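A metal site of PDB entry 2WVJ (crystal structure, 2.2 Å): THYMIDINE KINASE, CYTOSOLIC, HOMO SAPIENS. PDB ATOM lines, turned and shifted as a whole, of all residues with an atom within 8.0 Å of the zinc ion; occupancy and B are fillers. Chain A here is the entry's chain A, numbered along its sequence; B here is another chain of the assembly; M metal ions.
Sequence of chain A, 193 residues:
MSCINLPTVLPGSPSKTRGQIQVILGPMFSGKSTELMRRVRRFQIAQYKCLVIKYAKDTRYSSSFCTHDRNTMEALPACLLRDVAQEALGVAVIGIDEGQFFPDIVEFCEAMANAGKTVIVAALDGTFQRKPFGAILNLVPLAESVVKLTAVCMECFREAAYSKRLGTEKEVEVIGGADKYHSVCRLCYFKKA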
ATOM      1  N   VAL A 152      -4.873   1.691  -9.511  1.00  0.00           N
ATOM      2  CA  VAL A 152      -3.956   0.613  -9.908  1.00  0.00           C
ATOM      3  C   VAL A 152      -3.412   0.945 -11.308  1.00  0.00           C
ATOM      4  O   VAL A 152      -4.183   1.329 -12.193  1.00  0.00           O
ATOM      5  CB  VAL A 152      -4.655  -0.785  -9.874  1.00  0.00           C
ATOM      6  CG1 VAL A 152      -3.707  -1.891 -10.345  1.00  0.00           C
ATOM      7  CG2 VAL A 152      -5.175  -1.090  -8.464  1.00  0.00           C
ATOM      8  N   CYS A 153      -2.090   0.824 -11.471  1.00  0.00           N
ATOM      9  CA  CYS A 153      -1.441   1.012 -12.775  1.00  0.00           C
ATOM     10  C   CYS A 153      -1.936  -0.061 -13.735  1.00  0.00           C
ATOM     11  O   CYS A 153      -1.769  -1.249 -13.478  1.00  0.00           O
ATOM     12  CB  CYS A 153       0.092   0.960 -12.661  1.00  0.00           C
ATOM     13  SG  CYS A 153       1.002   1.178 -14.231  1.00  0.00           S
ATOM     14  N   MET A 154      -2.548   0.369 -14.831  1.00  0.00           N
ATOM     15  CA  MET A 154      -3.091  -0.562 -15.804  1.00  0.00           C
ATOM     16  C   MET A 154      -2.036  -1.238 -16.682  1.00  0.00           C
ATOM     17  O   MET A 154      -2.377  -2.073 -17.535  1.00  0.00           O
ATOM     18  CB  MET A 154      -4.146   0.138 -16.664  1.00  0.00           C
ATOM     19  CG  MET A 154      -5.419   0.445 -15.911  1.00  0.00           C
ATOM     20  SD  MET A 154      -6.413   1.648 -16.783  1.00  0.00           S
ATOM     21  CE  MET A 154      -7.907   1.591 -15.826  1.00  0.00           C
ATOM     22  N   GLU A 155      -0.766  -0.898 -16.478  1.00  0.00           N
ATOM     23  CA  GLU A 155       0.309  -1.460 -17.298  1.00  0.00           C
ATOM     24  C   GLU A 155       1.293  -2.378 -16.550  1.00  0.00           C
ATOM     25  O   GLU A 155       1.756  -3.362 -17.103  1.00  0.00           O
ATOM     26  CB  GLU A 155       1.036  -0.364 -18.073  1.00  0.00           C
ATOM     27  CG  GLU A 155       0.170   0.244 -19.178  1.00  0.00           C
ATOM     28  CD  GLU A 155       0.683   1.563 -19.705  1.00  0.00           C
ATOM     29  OE1 GLU A 155      -0.131   2.336 -20.265  1.00  0.00           O
ATOM     30  OE2 GLU A 155       1.898   1.841 -19.585  1.00  0.00           O
ATOM     31  N   CYS A 156       1.595  -2.047 -15.296  1.00  0.00           N
ATOM     32  CA  CYS A 156       2.474  -2.896 -14.464  1.00  0.00           C
ATOM     33  C   CYS A 156       1.779  -3.356 -13.178  1.00  0.00           C
ATOM     34  O   CYS A 156       2.325  -4.179 -12.442  1.00  0.00           O
ATOM     35  CB  CYS A 156       3.787  -2.180 -14.125  1.00  0.00           C
ATOM     36  SG  CYS A 156       3.686  -1.061 -12.709  1.00  0.00           S
ATOM     37  N   PHE A 157       0.600  -2.800 -12.914  1.00  0.00           N
ATOM     38  CA  PHE A 157      -0.259  -3.224 -11.797  1.00  0.00           C
ATOM     39  C   PHE A 157       0.278  -2.892 -10.388  1.00  0.00           C
ATOM     40  O   PHE A 157      -0.178  -3.443  -9.389  1.00  0.00           O
ATOM     41  CB  PHE A 157      -0.674  -4.694 -11.935  1.00  0.00           C
ATOM     42  CG  PHE A 157      -1.080  -5.059 -13.333  1.00  0.00           C
ATOM     43  CD1 PHE A 157      -0.259  -5.863 -14.130  1.00  0.00           C
ATOM     44  CD2 PHE A 157      -2.257  -4.559 -13.872  1.00  0.00           C
ATOM     45  CE1 PHE A 157      -0.625  -6.183 -15.425  1.00  0.00           C
ATOM     46  CE2 PHE A 157      -2.640  -4.870 -15.173  1.00  0.00           C
ATOM     47  CZ  PHE A 157      -1.822  -5.691 -15.951  1.00  0.00           C
ATOM     48  N   ARG A 158       1.235  -1.970 -10.329  1.00  0.00           N
ATOM     49  CA  ARG A 158       1.593  -1.351  -9.064  1.00  0.00           C
ATOM     50  C   ARG A 158       0.652  -0.171  -8.793  1.00  0.00           C
ATOM     51  O   ARG A 158      -0.348  -0.004  -9.499  1.00  0.00           O
ATOM     52  CB  ARG A 158       3.051  -0.926  -9.056  1.00  0.00           C
ATOM     53  CG  ARG A 158       4.008  -2.088  -8.880  1.00  0.00           C
ATOM     54  CD  ARG A 158       5.453  -1.646  -8.881  1.00  0.00           C
ATOM     55  NE  ARG A 158       6.359  -2.768  -8.661  1.00  0.00           N
ATOM     56  CZ  ARG A 158       6.821  -3.574  -9.630  1.00  0.00           C
ATOM     57  NH1 ARG A 158       6.464  -3.375 -10.892  1.00  0.00           N
ATOM     58  NH2 ARG A 158       7.637  -4.571  -9.318  1.00  0.00           N
ATOM     59  N   GLU A 159       0.973   0.630  -7.782  1.00  0.00           N
ATOM     60  CA  GLU A 159       0.148   1.772  -7.421  1.00  0.00           C
ATOM     61  C   GLU A 159       0.312   2.905  -8.442  1.00  0.00           C
ATOM     62  O   GLU A 159       1.423   3.210  -8.860  1.00  0.00           O
ATOM     63  CB  GLU A 159       0.538   2.260  -6.026  1.00  0.00           C
ATOM     64  CG  GLU A 159      -0.589   2.902  -5.280  1.00  0.00           C
ATOM     65  CD  GLU A 159      -0.410   2.835  -3.779  1.00  0.00           C
ATOM     66  OE1 GLU A 159       0.636   3.280  -3.270  1.00  0.00           O
ATOM     67  OE2 GLU A 159      -1.333   2.323  -3.110  1.00  0.00           O
ATOM     68  N   ALA A 160      -0.808   3.506  -8.838  1.00  0.00           N
ATOM     69  CA  ALA A 160      -0.841   4.548  -9.871  1.00  0.00           C
ATOM     70  C   ALA A 160      -1.258   5.914  -9.340  1.00  0.00           C
ATOM     71  O   ALA A 160      -2.259   6.044  -8.634  1.00  0.00           O
ATOM     72  CB  ALA A 160      -1.736   4.134 -11.017  1.00  0.00           C
ATOM     73  N   SER A 183      -4.613   4.814 -15.976  1.00  0.00           N
ATOM     74  CA  SER A 183      -3.988   5.171 -14.696  1.00  0.00           C
ATOM     75  C   SER A 183      -2.628   4.482 -14.666  1.00  0.00           C
ATOM     76  O   SER A 183      -2.541   3.298 -14.991  1.00  0.00           O
ATOM     77  CB  SER A 183      -4.861   4.733 -13.517  1.00  0.00           C
ATOM     78  OG  SER A 183      -5.209   3.357 -13.597  1.00  0.00           O
ATOM     79  N   VAL A 184      -1.569   5.226 -14.331  1.00  0.00           N
ATOM     80  CA  VAL A 184      -0.197   4.711 -14.383  1.00  0.00           C
ATOM     81  C   VAL A 184       0.691   5.186 -13.222  1.00  0.00           C
ATOM     82  O   VAL A 184       0.465   6.255 -12.641  1.00  0.00           O
ATOM     83  CB  VAL A 184       0.541   5.065 -15.728  1.00  0.00           C
ATOM     84  CG1 VAL A 184      -0.091   4.324 -16.928  1.00  0.00           C
ATOM     85  CG2 VAL A 184       0.566   6.586 -15.954  1.00  0.00           C
ATOM     86  N   CYS A 185       1.708   4.386 -12.915  1.00  0.00           N
ATOM     87  CA  CYS A 185       2.785   4.798 -12.024  1.00  0.00           C
ATOM     88  C   CYS A 185       3.773   5.690 -12.779  1.00  0.00           C
ATOM     89  O   CYS A 185       3.630   5.922 -13.991  1.00  0.00           O
ATOM     90  CB  CYS A 185       3.506   3.561 -11.472  1.00  0.00           C
ATOM     91  SG  CYS A 185       4.388   2.619 -12.754  1.00  0.00           S
ATOM     92  N   ARG A 186       4.792   6.175 -12.070  1.00  0.00           N
ATOM     93  CA  ARG A 186       5.806   7.056 -12.663  1.00  0.00           C
ATOM     94  C   ARG A 186       6.556   6.398 -13.820  1.00  0.00           C
ATOM     95  O   ARG A 186       6.685   6.992 -14.900  1.00  0.00           O
ATOM     96  CB  ARG A 186       6.786   7.525 -11.583  1.00  0.00           C
ATOM     97  CG  ARG A 186       7.939   8.394 -12.109  1.00  0.00           C
ATOM     98  CD  ARG A 186       8.832   8.844 -10.969  1.00  0.00           C
ATOM     99  NE  ARG A 186       8.101   9.654  -9.994  1.00  0.00           N
ATOM    100  CZ  ARG A 186       8.069  10.985  -9.980  1.00  0.00           C
ATOM    101  NH1 ARG A 186       8.751  11.685 -10.881  1.00  0.00           N
ATOM    102  NH2 ARG A 186       7.371  11.613  -9.049  1.00  0.00           N
ATOM    103  N   LEU A 187       7.043   5.174 -13.596  1.00  0.00           N
ATOM    104  CA  LEU A 187       7.834   4.442 -14.593  1.00  0.00           C
ATOM    105  C   LEU A 187       7.057   4.171 -15.878  1.00  0.00           C
ATOM    106  O   LEU A 187       7.586   4.365 -16.970  1.00  0.00           O
ATOM    107  CB  LEU A 187       8.382   3.138 -14.019  1.00  0.00           C
ATOM    108  CG  LEU A 187       9.311   3.215 -12.801  1.00  0.00           C
ATOM    109  CD1 LEU A 187       9.875   1.840 -12.480  1.00  0.00           C
ATOM    110  CD2 LEU A 187      10.442   4.225 -13.007  1.00  0.00           C
ATOM    111  N   CYS A 188       5.804   3.748 -15.744  1.00  0.00           N
ATOM    112  CA  CYS A 188       4.958   3.462 -16.903  1.00  0.00           C
ATOM    113  C   CYS A 188       4.542   4.715 -17.657  1.00  0.00           C
ATOM    114  O   CYS A 188       4.380   4.686 -18.880  1.00  0.00           O
ATOM    115  CB  CYS A 188       3.737   2.636 -16.501  1.00  0.00           C
ATOM    116  SG  CYS A 188       4.148   0.920 -16.083  1.00  0.00           S
ATOM    117  N   TYR A 189       4.368   5.815 -16.922  1.00  0.00           N
ATOM    118  CA  TYR A 189       4.086   7.120 -17.528  1.00  0.00           C
ATOM    119  C   TYR A 189       5.172   7.508 -18.528  1.00  0.00           C
ATOM    120  O   TYR A 189       4.863   7.943 -19.644  1.00  0.00           O
ATOM    121  CB  TYR A 189       3.934   8.216 -16.447  1.00  0.00           C
ATOM    122  CG  TYR A 189       3.517   9.554 -17.008  1.00  0.00           C
ATOM    123  CD1 TYR A 189       2.171   9.868 -17.203  1.00  0.00           C
ATOM    124  CD2 TYR A 189       4.469  10.506 -17.385  1.00  0.00           C
ATOM    125  CE1 TYR A 189       1.779  11.077 -17.726  1.00  0.00           C
ATOM    126  CE2 TYR A 189       4.093  11.740 -17.917  1.00  0.00           C
ATOM    127  CZ  TYR A 189       2.742  12.017 -18.084  1.00  0.00           C
ATOM    128  OH  TYR A 189       2.354  13.215 -18.601  1.00  0.00           O
ATOM    129  N   LYS A 191       7.215   5.734 -20.265  1.00  0.00           N
ATOM    130  CA  LYS A 191       7.543   4.739 -21.285  1.00  0.00           C
ATOM    131  C   LYS A 191       7.152   5.270 -22.661  1.00  0.00           C
ATOM    132  O   LYS A 191       5.989   5.189 -23.070  1.00  0.00           O
ATOM    133  CB  LYS A 191       6.851   3.405 -21.004  1.00  0.00           C
ATOM    134  CG  LYS A 191       7.414   2.657 -19.805  1.00  0.00           C
ATOM    135  CD  LYS A 191       7.099   1.178 -19.867  1.00  0.00           C
ATOM    136  CE  LYS A 191       7.793   0.413 -18.742  1.00  0.00           C
ATOM    137  NZ  LYS A 191       9.275   0.625 -18.687  1.00  0.00           N
ATOM    138  N   ARG B  18      13.076   2.759  -8.289  1.00  0.00           N
ATOM    139  CA  ARG B  18      11.681   3.288  -8.212  1.00  0.00           C
ATOM    140  C   ARG B  18      11.586   4.550  -7.338  1.00  0.00           C
ATOM    141  O   ARG B  18      11.294   4.490  -6.131  1.00  0.00           O
ATOM    142  CB  ARG B  18      10.691   2.213  -7.735  1.00  0.00           C
ATOM    143  CG  ARG B  18      10.473   1.098  -8.749  1.00  0.00           C
ATOM    144  CD  ARG B  18       9.173   0.357  -8.479  1.00  0.00           C
ATOM    145  NE  ARG B  18       8.013   1.106  -8.946  1.00  0.00           N
ATOM    146  CZ  ARG B  18       7.329   0.823 -10.055  1.00  0.00           C
ATOM    147  NH1 ARG B  18       7.667  -0.210 -10.824  1.00  0.00           N
ATOM    148  NH2 ARG B  18       6.290   1.583 -10.399  1.00  0.00           N
HETATM  149 ZN    ZN M   1       3.230   0.942 -13.828  1.00  0.00          ZN
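N of Glu 155 sits close to SG of Cys 153, 3.5 Å away.
The guanidinium group (NH2) of Arg 18 of chain B lies close to the side-chain sulfur (SG) of Cys 185 (3.2 Å).
N of Cys 153 lies within hydrogen-bond range of O of Arg 158 (2.8 Å).
The side-chain sulfur (SG) of Cys 185 lies close to the backbone NH (N) of Leu 187 (3.8 Å).
The backbone NH of Arg 158 lies close to the side-chain sulfur of Cys 156.
Of the 18 residues printed, 4 come within 4 Å of the zinc ion.
The nearest printed residue that does not touch the zinc ion is Arg 18 of chain B (4.6 Å).
The zinc ion is bound by SG of Cys 153 (2.3 Å), SG of Cys 185 (2.3 Å), SG of Cys 156 (2.3 Å) and SG of Cys 188 (2.4 Å).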
